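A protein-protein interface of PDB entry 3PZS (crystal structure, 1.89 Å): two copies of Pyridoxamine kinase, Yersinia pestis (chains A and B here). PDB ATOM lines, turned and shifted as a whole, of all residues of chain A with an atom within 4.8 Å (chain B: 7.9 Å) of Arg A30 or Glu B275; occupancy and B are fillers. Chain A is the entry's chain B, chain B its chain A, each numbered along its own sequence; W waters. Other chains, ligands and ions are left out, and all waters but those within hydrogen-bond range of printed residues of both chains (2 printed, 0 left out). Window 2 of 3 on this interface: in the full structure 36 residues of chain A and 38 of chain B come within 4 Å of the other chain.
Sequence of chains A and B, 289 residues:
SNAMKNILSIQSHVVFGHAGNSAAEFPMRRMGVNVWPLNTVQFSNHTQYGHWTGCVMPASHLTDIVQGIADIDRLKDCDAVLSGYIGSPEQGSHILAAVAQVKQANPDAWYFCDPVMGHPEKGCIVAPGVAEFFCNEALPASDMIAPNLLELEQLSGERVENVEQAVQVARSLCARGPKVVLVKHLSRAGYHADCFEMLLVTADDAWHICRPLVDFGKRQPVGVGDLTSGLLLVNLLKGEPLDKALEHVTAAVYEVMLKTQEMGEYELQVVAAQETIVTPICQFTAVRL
Arg A30 touches just these residues of chain B: Phe B26, Arg B30, Gln B274 and Glu B275.
Of the printed residues of chain A, Phe B26 touches Phe A26 (3.6 Å), Arg A29 (3.6 Å) and Arg A30 (3.7 Å).
Printed residues of chain A within 4 Å of Arg B29: Phe A26 (3.6 Å) and Gln A274 (3.2 Å).
Printed residues of chain A within 4 Å of Arg B30: Phe A26 (3.8 Å), Arg A30 (3.4 Å), Gln A274 (3.6 Å) and Glu A275 (3.9 Å).
Printed residues of chain A within 4 Å of Val B271: Arg A29.
Glu B275 touches one residue of chain A.
The nearest residue of chain B that does not touch Arg A30 is Val B271 (5.5 Å).
The nearest printed residue of chain A that does not touch Glu B275 is Glu A275 (6.7 Å).
Printed residues of chain B that touch a printed residue of chain A: Phe B26, Arg B29, Arg B30, Val B271, Gln B274 and Glu B275.
Along chain B the printed residues that touch a printed residue of chain A span positions 26 to 275.
Hydrophobic or aromatic side chains of chain A within 4 Å of the printed part of chain B: Phe A26.
Among the printed residues, 14 pairs touch across the chains.
The side-chain amide nitrogen (NE2) of Gln A274 sits at hydrogen-bond distance from the backbone carbonyl oxygen (O) of Arg B29, 3.2 Å away.
NH1 of Arg B30 lies within salt-bridge range of OE2 of Glu A275.
The side-chain amide nitrogen (NE2) of Gln B274 lies within hydrogen-bond range of the backbone carbonyl oxygen (O) of Arg A29 (3.2 Å).
OE1 of Gln B274 is in hydrogen-bond range of NH1 of Arg A30.
The guanidinium group of Arg A30 lies within salt-bridge range of the side-chain carboxylate of Glu B275.
The guanidinium group of Arg A30 sits close to the guanidinium group of Arg B30 (3.4 Å).
Water W1 bridges the guanidinium group of Arg B30 and the side-chain carboxylate of Glu A275.
Water W2 lies within hydrogen-bond range of the guanidinium group of Arg A30 (2.9 Å) and the side-chain carboxylate of Glu B275 (3.2 Å).
Among the printed residues, pairs that only touch across the chains: Arg A29 with Val B271 (3.5 Å), Gln A274 with Arg B30 (3.6 Å), Phe A26 with Phe B26 (3.6 Å), Arg A29 with Phe B26 (3.6 Å), Phe A26 with Arg B29 (3.6 Å), Arg A30 with Phe B26 (3.7 Å), Phe A26 with Arg B30 (3.8 Å) and Gly A32 with Gln B274 (3.99 Å).
Phe A26 touches Arg B29, and with the chains exchanged Arg A29 touches Phe B26.
Phe A26 touches Arg B30, and with the chains exchanged Arg A30 touches Phe B26.
Arg A30 touches its own counterpart, Arg B30.
Arg A30 touches Glu B275, and with the chains exchanged Glu A275 touches Arg B30.
NE of Arg B30 sits at hydrogen-bond distance from OE1 of Gln B274, at 2.8 Å.
The guanidinium group of Arg B30 is in salt-bridge range of the side-chain carboxylate of Glu B275.
O of Val B271 sits close to NE2 of Gln B274, 3.4 Å away.
OE1 of Gln A274 is in hydrogen-bond range of NE of Arg A30.
The guanidinium group of Arg A30 lies within salt-bridge range of the side-chain carboxylate of Glu A275 (2.8 Å).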
ATOM      1  N   PHE A  26     -35.123 -30.731  24.640  1.00  0.00           N
ATOM      2  CA  PHE A  26     -34.211 -29.847  23.898  1.00  0.00           C
ATOM      3  C   PHE A  26     -32.757 -29.964  24.473  1.00  0.00           C
ATOM      4  O   PHE A  26     -31.846 -30.209  23.679  1.00  0.00           O
ATOM      5  CB  PHE A  26     -34.724 -28.378  23.832  1.00  0.00           C
ATOM      6  CG  PHE A  26     -33.662 -27.460  23.270  1.00  0.00           C
ATOM      7  CD1 PHE A  26     -33.402 -27.424  21.902  1.00  0.00           C
ATOM      8  CD2 PHE A  26     -32.833 -26.731  24.117  1.00  0.00           C
ATOM      9  CE1 PHE A  26     -32.378 -26.619  21.386  1.00  0.00           C
ATOM     10  CE2 PHE A  26     -31.815 -25.921  23.600  1.00  0.00           C
ATOM     11  CZ  PHE A  26     -31.595 -25.877  22.243  1.00  0.00           C
ATOM     12  N   PRO A  27     -32.507 -29.910  25.803  1.00  0.00           N
ATOM     13  CA  PRO A  27     -31.128 -30.109  26.299  1.00  0.00           C
ATOM     14  C   PRO A  27     -30.505 -31.446  25.894  1.00  0.00           C
ATOM     15  O   PRO A  27     -29.334 -31.479  25.534  1.00  0.00           O
ATOM     16  CB  PRO A  27     -31.303 -30.034  27.811  1.00  0.00           C
ATOM     17  CG  PRO A  27     -32.464 -29.044  27.973  1.00  0.00           C
ATOM     18  CD  PRO A  27     -33.416 -29.571  26.926  1.00  0.00           C
ATOM     19  N   MET A  28     -31.279 -32.544  25.879  1.00  0.00           N
ATOM     20  CA  MET A  28     -30.705 -33.845  25.517  1.00  0.00           C
ATOM     21  C   MET A  28     -30.349 -33.887  24.046  1.00  0.00           C
ATOM     22  O   MET A  28     -29.271 -34.381  23.708  1.00  0.00           O
ATOM     23  CB  MET A  28     -31.666 -34.978  25.907  1.00  0.00           C
ATOM     24  CG  MET A  28     -31.856 -35.094  27.462  1.00  0.00           C
ATOM     25  SD  MET A  28     -32.793 -36.741  27.960  1.00  0.00           S
ATOM     26  CE  MET A  28     -34.520 -36.452  27.161  1.00  0.00           C
ATOM     27  N   ARG A  29     -31.212 -33.329  23.160  1.00  0.00           N
ATOM     28  CA  ARG A  29     -30.916 -33.257  21.718  1.00  0.00           C
ATOM     29  C   ARG A  29     -29.736 -32.303  21.449  1.00  0.00           C
ATOM     30  O   ARG A  29     -28.883 -32.588  20.597  1.00  0.00           O
ATOM     31  CB  ARG A  29     -32.149 -32.790  20.942  1.00  0.00           C
ATOM     32  CG  ARG A  29     -33.203 -33.870  20.793  1.00  0.00           C
ATOM     33  CD  ARG A  29     -34.402 -33.315  20.068  1.00  0.00           C
ATOM     34  NE  ARG A  29     -35.255 -34.391  19.558  1.00  0.00           N
ATOM     35  CZ  ARG A  29     -36.547 -34.257  19.288  1.00  0.00           C
ATOM     36  NH1 ARG A  29     -37.158 -33.096  19.499  1.00  0.00           N
ATOM     37  NH2 ARG A  29     -37.242 -35.285  18.802  1.00  0.00           N
ATOM     38  N   ARG A  30     -29.652 -31.205  22.231  1.00  0.00           N
ATOM     39  CA  ARG A  30     -28.543 -30.225  22.152  1.00  0.00           C
ATOM     40  C   ARG A  30     -27.167 -30.904  22.435  1.00  0.00           C
ATOM     41  O   ARG A  30     -26.136 -30.484  21.880  1.00  0.00           O
ATOM     42  CB  ARG A  30     -28.800 -29.059  23.132  1.00  0.00           C
ATOM     43  CG  ARG A  30     -27.847 -27.868  22.967  1.00  0.00           C
ATOM     44  CD  ARG A  30     -27.880 -27.225  21.573  1.00  0.00           C
ATOM     45  NE  ARG A  30     -26.924 -26.111  21.496  1.00  0.00           N
ATOM     46  CZ  ARG A  30     -25.623 -26.248  21.270  1.00  0.00           C
ATOM     47  NH1 ARG A  30     -25.108 -27.443  21.014  1.00  0.00           N
ATOM     48  NH2 ARG A  30     -24.832 -25.184  21.256  1.00  0.00           N
ATOM     49  N   MET A  31     -27.162 -31.963  23.254  1.00  0.00           N
ATOM     50  CA  MET A  31     -25.941 -32.700  23.576  1.00  0.00           C
ATOM     51  C   MET A  31     -25.611 -33.763  22.509  1.00  0.00           C
ATOM     52  O   MET A  31     -24.589 -34.440  22.613  1.00  0.00           O
ATOM     53  CB  MET A  31     -26.066 -33.350  24.954  1.00  0.00           C
ATOM     54  CG  MET A  31     -26.132 -32.340  26.077  1.00  0.00           C
ATOM     55  SD  MET A  31     -25.888 -33.209  27.766  1.00  0.00           S
ATOM     56  CE  MET A  31     -24.020 -33.887  27.526  1.00  0.00           C
ATOM     57  N   GLY A  32     -26.458 -33.884  21.492  1.00  0.00           N
ATOM     58  CA  GLY A  32     -26.228 -34.810  20.378  1.00  0.00           C
ATOM     59  C   GLY A  32     -26.787 -36.211  20.501  1.00  0.00           C
ATOM     60  O   GLY A  32     -26.290 -37.131  19.842  1.00  0.00           O
ATOM     61  N   GLN A 274     -28.540 -22.690  26.330  1.00  0.00           N
ATOM     62  CA  GLN A 274     -28.083 -23.863  25.547  1.00  0.00           C
ATOM     63  C   GLN A 274     -26.562 -23.985  25.361  1.00  0.00           C
ATOM     64  O   GLN A 274     -26.065 -25.111  25.361  1.00  0.00           O
ATOM     65  CB  GLN A 274     -28.773 -23.958  24.179  1.00  0.00           C
ATOM     66  CG  GLN A 274     -28.430 -22.828  23.182  1.00  0.00           C
ATOM     67  CD  GLN A 274     -29.113 -23.074  21.866  1.00  0.00           C
ATOM     68  OE1 GLN A 274     -28.817 -24.038  21.162  1.00  0.00           O
ATOM     69  NE2 GLN A 274     -30.052 -22.208  21.515  1.00  0.00           N
ATOM     70  N   GLU A 275     -25.831 -22.857  25.215  1.00  0.00           N
ATOM     71  CA  GLU A 275     -24.372 -22.914  25.017  1.00  0.00           C
ATOM     72  C   GLU A 275     -23.672 -23.426  26.288  1.00  0.00           C
ATOM     73  O   GLU A 275     -22.729 -24.211  26.183  1.00  0.00           O
ATOM     74  CB  GLU A 275     -23.806 -21.547  24.586  1.00  0.00           C
ATOM     75  CG  GLU A 275     -24.346 -21.068  23.239  1.00  0.00           C
ATOM     76  CD  GLU A 275     -24.188 -22.056  22.092  1.00  0.00           C
ATOM     77  OE1 GLU A 275     -23.035 -22.468  21.824  1.00  0.00           O
ATOM     78  OE2 GLU A 275     -25.221 -22.460  21.501  1.00  0.00           O
ATOM     79  N   VAL A 278     -23.998 -27.522  26.847  1.00  0.00           N
ATOM     80  CA  VAL A 278     -22.964 -28.352  26.230  1.00  0.00           C
ATOM     81  C   VAL A 278     -21.597 -28.004  26.854  1.00  0.00           C
ATOM     82  O   VAL A 278     -20.870 -28.922  27.209  1.00  0.00           O
ATOM     83  CB  VAL A 278     -22.953 -28.264  24.675  1.00  0.00           C
ATOM     84  CG1 VAL A 278     -21.838 -29.120  24.082  1.00  0.00           C
ATOM     85  CG2 VAL A 278     -24.299 -28.710  24.106  1.00  0.00           C
ATOM     86  N   PHE B  26     -36.882 -28.553  17.195  1.00  0.00           N
ATOM     87  CA  PHE B  26     -35.473 -28.546  17.636  1.00  0.00           C
ATOM     88  C   PHE B  26     -34.656 -27.502  16.817  1.00  0.00           C
ATOM     89  O   PHE B  26     -34.027 -26.639  17.441  1.00  0.00           O
ATOM     90  CB  PHE B  26     -34.823 -29.956  17.620  1.00  0.00           C
ATOM     91  CG  PHE B  26     -33.330 -29.898  17.882  1.00  0.00           C
ATOM     92  CD1 PHE B  26     -32.839 -29.693  19.169  1.00  0.00           C
ATOM     93  CD2 PHE B  26     -32.419 -29.993  16.831  1.00  0.00           C
ATOM     94  CE1 PHE B  26     -31.465 -29.609  19.404  1.00  0.00           C
ATOM     95  CE2 PHE B  26     -31.046 -29.905  17.066  1.00  0.00           C
ATOM     96  CZ  PHE B  26     -30.576 -29.706  18.347  1.00  0.00           C
ATOM     97  N   ARG B  29     -35.471 -23.900  18.005  1.00  0.00           N
ATOM     98  CA  ARG B  29     -34.889 -23.654  19.337  1.00  0.00           C
ATOM     99  C   ARG B  29     -33.357 -23.569  19.231  1.00  0.00           C
ATOM    100  O   ARG B  29     -32.733 -22.774  19.930  1.00  0.00           O
ATOM    101  CB  ARG B  29     -35.283 -24.759  20.336  1.00  0.00           C
ATOM    102  CG  ARG B  29     -36.708 -24.617  20.821  1.00  0.00           C
ATOM    103  CD  ARG B  29     -37.093 -25.783  21.684  1.00  0.00           C
ATOM    104  NE  ARG B  29     -38.335 -25.517  22.406  1.00  0.00           N
ATOM    105  CZ  ARG B  29     -39.096 -26.452  22.955  1.00  0.00           C
ATOM    106  NH1 ARG B  29     -38.783 -27.735  22.822  1.00  0.00           N
ATOM    107  NH2 ARG B  29     -40.192 -26.112  23.626  1.00  0.00           N
ATOM    108  N   ARG B  30     -32.750 -24.390  18.345  1.00  0.00           N
ATOM    109  CA  ARG B  30     -31.288 -24.369  18.123  1.00  0.00           C
ATOM    110  C   ARG B  30     -30.824 -22.967  17.645  1.00  0.00           C
ATOM    111  O   ARG B  30     -29.696 -22.542  17.943  1.00  0.00           O
ATOM    112  CB  ARG B  30     -30.883 -25.479  17.122  1.00  0.00           C
ATOM    113  CG  ARG B  30     -29.371 -25.741  17.007  1.00  0.00           C
ATOM    114  CD  ARG B  30     -28.706 -26.174  18.321  1.00  0.00           C
ATOM    115  NE  ARG B  30     -27.263 -26.384  18.138  1.00  0.00           N
ATOM    116  CZ  ARG B  30     -26.349 -25.420  18.078  1.00  0.00           C
ATOM    117  NH1 ARG B  30     -26.696 -24.151  18.252  1.00  0.00           N
ATOM    118  NH2 ARG B  30     -25.075 -25.720  17.883  1.00  0.00           N
ATOM    119  N   MET B  31     -31.719 -22.257  16.938  1.00  0.00           N
ATOM    120  CA  MET B  31     -31.512 -20.902  16.417  1.00  0.00           C
ATOM    121  C   MET B  31     -31.758 -19.801  17.486  1.00  0.00           C
ATOM    122  O   MET B  31     -31.669 -18.619  17.164  1.00  0.00           O
ATOM    123  CB  MET B  31     -32.430 -20.660  15.211  1.00  0.00           C
ATOM    124  CG  MET B  31     -32.099 -21.505  13.997  1.00  0.00           C
ATOM    125  SD  MET B  31     -30.504 -20.861  13.100  1.00  0.00           S
ATOM    126  CE  MET B  31     -31.155 -19.051  12.510  1.00  0.00           C
ATOM    127  N   HIS B 248     -29.725 -18.156   4.206  1.00  0.00           N
ATOM    128  CA  HIS B 248     -29.534 -19.022   5.374  1.00  0.00           C
ATOM    129  C   HIS B 248     -30.470 -20.222   5.306  1.00  0.00           C
ATOM    130  O   HIS B 248     -30.009 -21.355   5.444  1.00  0.00           O
ATOM    131  CB  HIS B 248     -29.738 -18.257   6.700  1.00  0.00           C
ATOM    132  CG  HIS B 248     -29.674 -19.188   7.874  1.00  0.00           C
ATOM    133  ND1 HIS B 248     -30.814 -19.819   8.353  1.00  0.00           N
ATOM    134  CD2 HIS B 248     -28.593 -19.691   8.515  1.00  0.00           C
ATOM    135  CE1 HIS B 248     -30.396 -20.647   9.297  1.00  0.00           C
ATOM    136  NE2 HIS B 248     -29.068 -20.599   9.440  1.00  0.00           N
ATOM    137  N   GLU B 255     -27.988 -28.520   4.152  1.00  0.00           N
ATOM    138  CA  GLU B 255     -27.041 -29.185   5.070  1.00  0.00           C
ATOM    139  C   GLU B 255     -27.687 -30.357   5.799  1.00  0.00           C
ATOM    140  O   GLU B 255     -27.050 -31.405   5.978  1.00  0.00           O
ATOM    141  CB  GLU B 255     -26.482 -28.193   6.088  1.00  0.00           C
ATOM    142  CG  GLU B 255     -25.506 -27.204   5.483  1.00  0.00           C
ATOM    143  CD  GLU B 255     -24.059 -27.639   5.440  1.00  0.00           C
ATOM    144  OE1 GLU B 255     -23.768 -28.854   5.530  1.00  0.00           O
ATOM    145  OE2 GLU B 255     -23.204 -26.734   5.351  1.00  0.00           O
ATOM    146  N   VAL B 270     -32.198 -33.811  11.666  1.00  0.00           N
ATOM    147  CA  VAL B 270     -32.173 -32.470  12.253  1.00  0.00           C
ATOM    148  C   VAL B 270     -31.222 -32.355  13.473  1.00  0.00           C
ATOM    149  O   VAL B 270     -30.708 -31.258  13.716  1.00  0.00           O
ATOM    150  CB  VAL B 270     -33.588 -31.913  12.589  1.00  0.00           C
ATOM    151  CG1 VAL B 270     -34.428 -31.721  11.327  1.00  0.00           C
ATOM    152  CG2 VAL B 270     -34.321 -32.766  13.631  1.00  0.00           C
ATOM    153  N   VAL B 271     -30.981 -33.449  14.225  1.00  0.00           N
ATOM    154  CA  VAL B 271     -30.117 -33.413  15.406  1.00  0.00           C
ATOM    155  C   VAL B 271     -28.637 -33.589  15.000  1.00  0.00           C
ATOM    156  O   VAL B 271     -27.790 -32.799  15.423  1.00  0.00           O
ATOM    157  CB  VAL B 271     -30.535 -34.423  16.520  1.00  0.00           C
ATOM    158  CG1 VAL B 271     -29.550 -34.363  17.706  1.00  0.00           C
ATOM    159  CG2 VAL B 271     -31.963 -34.133  17.002  1.00  0.00           C
ATOM    160  N   ALA B 272     -28.336 -34.589  14.158  1.00  0.00           N
ATOM    161  CA  ALA B 272     -26.967 -34.839  13.675  1.00  0.00           C
ATOM    162  C   ALA B 272     -26.386 -33.615  12.925  1.00  0.00           C
ATOM    163  O   ALA B 272     -25.197 -33.333  13.057  1.00  0.00           O
ATOM    164  CB  ALA B 272     -26.965 -36.056  12.763  1.00  0.00           C
ATOM    165  N   ALA B 273     -27.247 -32.837  12.232  1.00  0.00           N
ATOM    166  CA  ALA B 273     -26.861 -31.662  11.434  1.00  0.00           C
ATOM    167  C   ALA B 273     -27.009 -30.331  12.186  1.00  0.00           C
ATOM    168  O   ALA B 273     -26.940 -29.281  11.556  1.00  0.00           O
ATOM    169  CB  ALA B 273     -27.716 -31.618  10.161  1.00  0.00           C
ATOM    170  N   GLN B 274     -27.203 -30.353  13.517  1.00  0.00           N
ATOM    171  CA  GLN B 274     -27.489 -29.127  14.289  1.00  0.00           C
ATOM    172  C   GLN B 274     -26.430 -28.019  14.157  1.00  0.00           C
ATOM    173  O   GLN B 274     -26.794 -26.847  14.138  1.00  0.00           O
ATOM    174  CB  GLN B 274     -27.721 -29.443  15.776  1.00  0.00           C
ATOM    175  CG  GLN B 274     -26.496 -29.937  16.545  1.00  0.00           C
ATOM    176  CD  GLN B 274     -26.850 -30.117  17.992  1.00  0.00           C
ATOM    177  OE1 GLN B 274     -27.103 -29.148  18.715  1.00  0.00           O
ATOM    178  NE2 GLN B 274     -26.915 -31.362  18.431  1.00  0.00           N
ATOM    179  N   GLU B 275     -25.137 -28.380  14.071  1.00  0.00           N
ATOM    180  CA  GLU B 275     -24.066 -27.378  13.940  1.00  0.00           C
ATOM    181  C   GLU B 275     -24.182 -26.596  12.616  1.00  0.00           C
ATOM    182  O   GLU B 275     -23.988 -25.380  12.607  1.00  0.00           O
ATOM    183  CB  GLU B 275     -22.665 -28.028  14.060  1.00  0.00           C
ATOM    184  CG  GLU B 275     -22.362 -28.618  15.427  1.00  0.00           C
ATOM    185  CD  GLU B 275     -22.637 -27.709  16.614  1.00  0.00           C
ATOM    186  OE1 GLU B 275     -22.071 -26.595  16.659  1.00  0.00           O
ATOM    187  OE2 GLU B 275     -23.451 -28.100  17.480  1.00  0.00           O
ATOM    188  N   THR B 276     -24.572 -27.277  11.534  1.00  0.00           N
ATOM    189  CA  THR B 276     -24.710 -26.663  10.210  1.00  0.00           C
ATOM    190  C   THR B 276     -26.079 -25.963  10.027  1.00  0.00           C
ATOM    191  O   THR B 276     -26.267 -25.273   9.029  1.00  0.00           O
ATOM    192  CB  THR B 276     -24.392 -27.680   9.125  1.00  0.00           C
ATOM    193  OG1 THR B 276     -25.219 -28.848   9.279  1.00  0.00           O
ATOM    194  CG2 THR B 276     -22.915 -28.083   9.148  1.00  0.00           C
ATOM    195  N   ILE B 277     -27.019 -26.098  10.996  1.00  0.00           N
ATOM    196  CA  ILE B 277     -28.293 -25.360  10.945  1.00  0.00           C
ATOM    197  C   ILE B 277     -27.987 -23.908  11.315  1.00  0.00           C
ATOM    198  O   ILE B 277     -28.414 -22.978  10.625  1.00  0.00           O
ATOM    199  CB  ILE B 277     -29.374 -25.995  11.880  1.00  0.00           C
ATOM    200  CG1 ILE B 277     -29.847 -27.364  11.326  1.00  0.00           C
ATOM    201  CG2 ILE B 277     -30.572 -25.022  12.094  1.00  0.00           C
ATOM    202  CD1 ILE B 277     -30.837 -28.189  12.224  1.00  0.00           C
ATOM    203  N   VAL B 278     -27.239 -23.705  12.414  1.00  0.00           N
ATOM    204  CA  VAL B 278     -26.917 -22.358  12.847  1.00  0.00           C
ATOM    205  C   VAL B 278     -25.876 -21.732  11.910  1.00  0.00           C
ATOM    206  O   VAL B 278     -26.050 -20.577  11.517  1.00  0.00           O
ATOM    207  CB  VAL B 278     -26.467 -22.315  14.333  1.00  0.00           C
ATOM    208  CG1 VAL B 278     -26.014 -20.909  14.731  1.00  0.00           C
ATOM    209  CG2 VAL B 278     -27.602 -22.783  15.250  1.00  0.00           C
ATOM    210  N   THR B 279     -24.816 -22.492  11.553  1.00  0.00           N
ATOM    211  CA  THR B 279     -23.736 -21.972  10.707  1.00  0.00           C
ATOM    212  C   THR B 279     -23.504 -22.892   9.511  1.00  0.00           C
ATOM    213  O   THR B 279     -22.614 -23.738   9.549  1.00  0.00           O
ATOM    214  CB  THR B 279     -22.441 -21.794  11.530  1.00  0.00           C
ATOM    215  OG1 THR B 279     -22.757 -21.303  12.835  1.00  0.00           O
ATOM    216  CG2 THR B 279     -21.440 -20.867  10.843  1.00  0.00           C
ATOM    217  N   PRO B 280     -24.296 -22.760   8.430  1.00  0.00           N
ATOM    218  CA  PRO B 280     -24.070 -23.630   7.263  1.00  0.00           C
ATOM    219  C   PRO B 280     -22.670 -23.436   6.653  1.00  0.00           C
ATOM    220  O   PRO B 280     -22.135 -22.330   6.696  1.00  0.00           O
ATOM    221  CB  PRO B 280     -25.158 -23.191   6.276  1.00  0.00           C
ATOM    222  CG  PRO B 280     -26.170 -22.454   7.097  1.00  0.00           C
ATOM    223  CD  PRO B 280     -25.412 -21.815   8.201  1.00  0.00           C
ATOM    224  N   ILE B 281     -22.058 -24.533   6.178  1.00  0.00           N
ATOM    225  CA  ILE B 281     -20.758 -24.537   5.491  1.00  0.00           C
ATOM    226  C   ILE B 281     -21.035 -24.146   4.027  1.00  0.00           C
ATOM    227  O   ILE B 281     -20.330 -23.309   3.463  1.00  0.00           O
ATOM    228  CB  ILE B 281     -20.031 -25.914   5.619  1.00  0.00           C
ATOM    229  CG1 ILE B 281     -19.858 -26.373   7.094  1.00  0.00           C
ATOM    230  CG2 ILE B 281     -18.700 -25.953   4.834  1.00  0.00           C
ATOM    231  CD1 ILE B 281     -18.921 -25.554   7.984  1.00  0.00           C
HETATM  232  O   HOH W   1     -24.574 -22.334  18.492  1.00  0.00           O
HETATM  233  O   HOH W   2     -22.518 -28.564  20.459  1.00  0.00           O
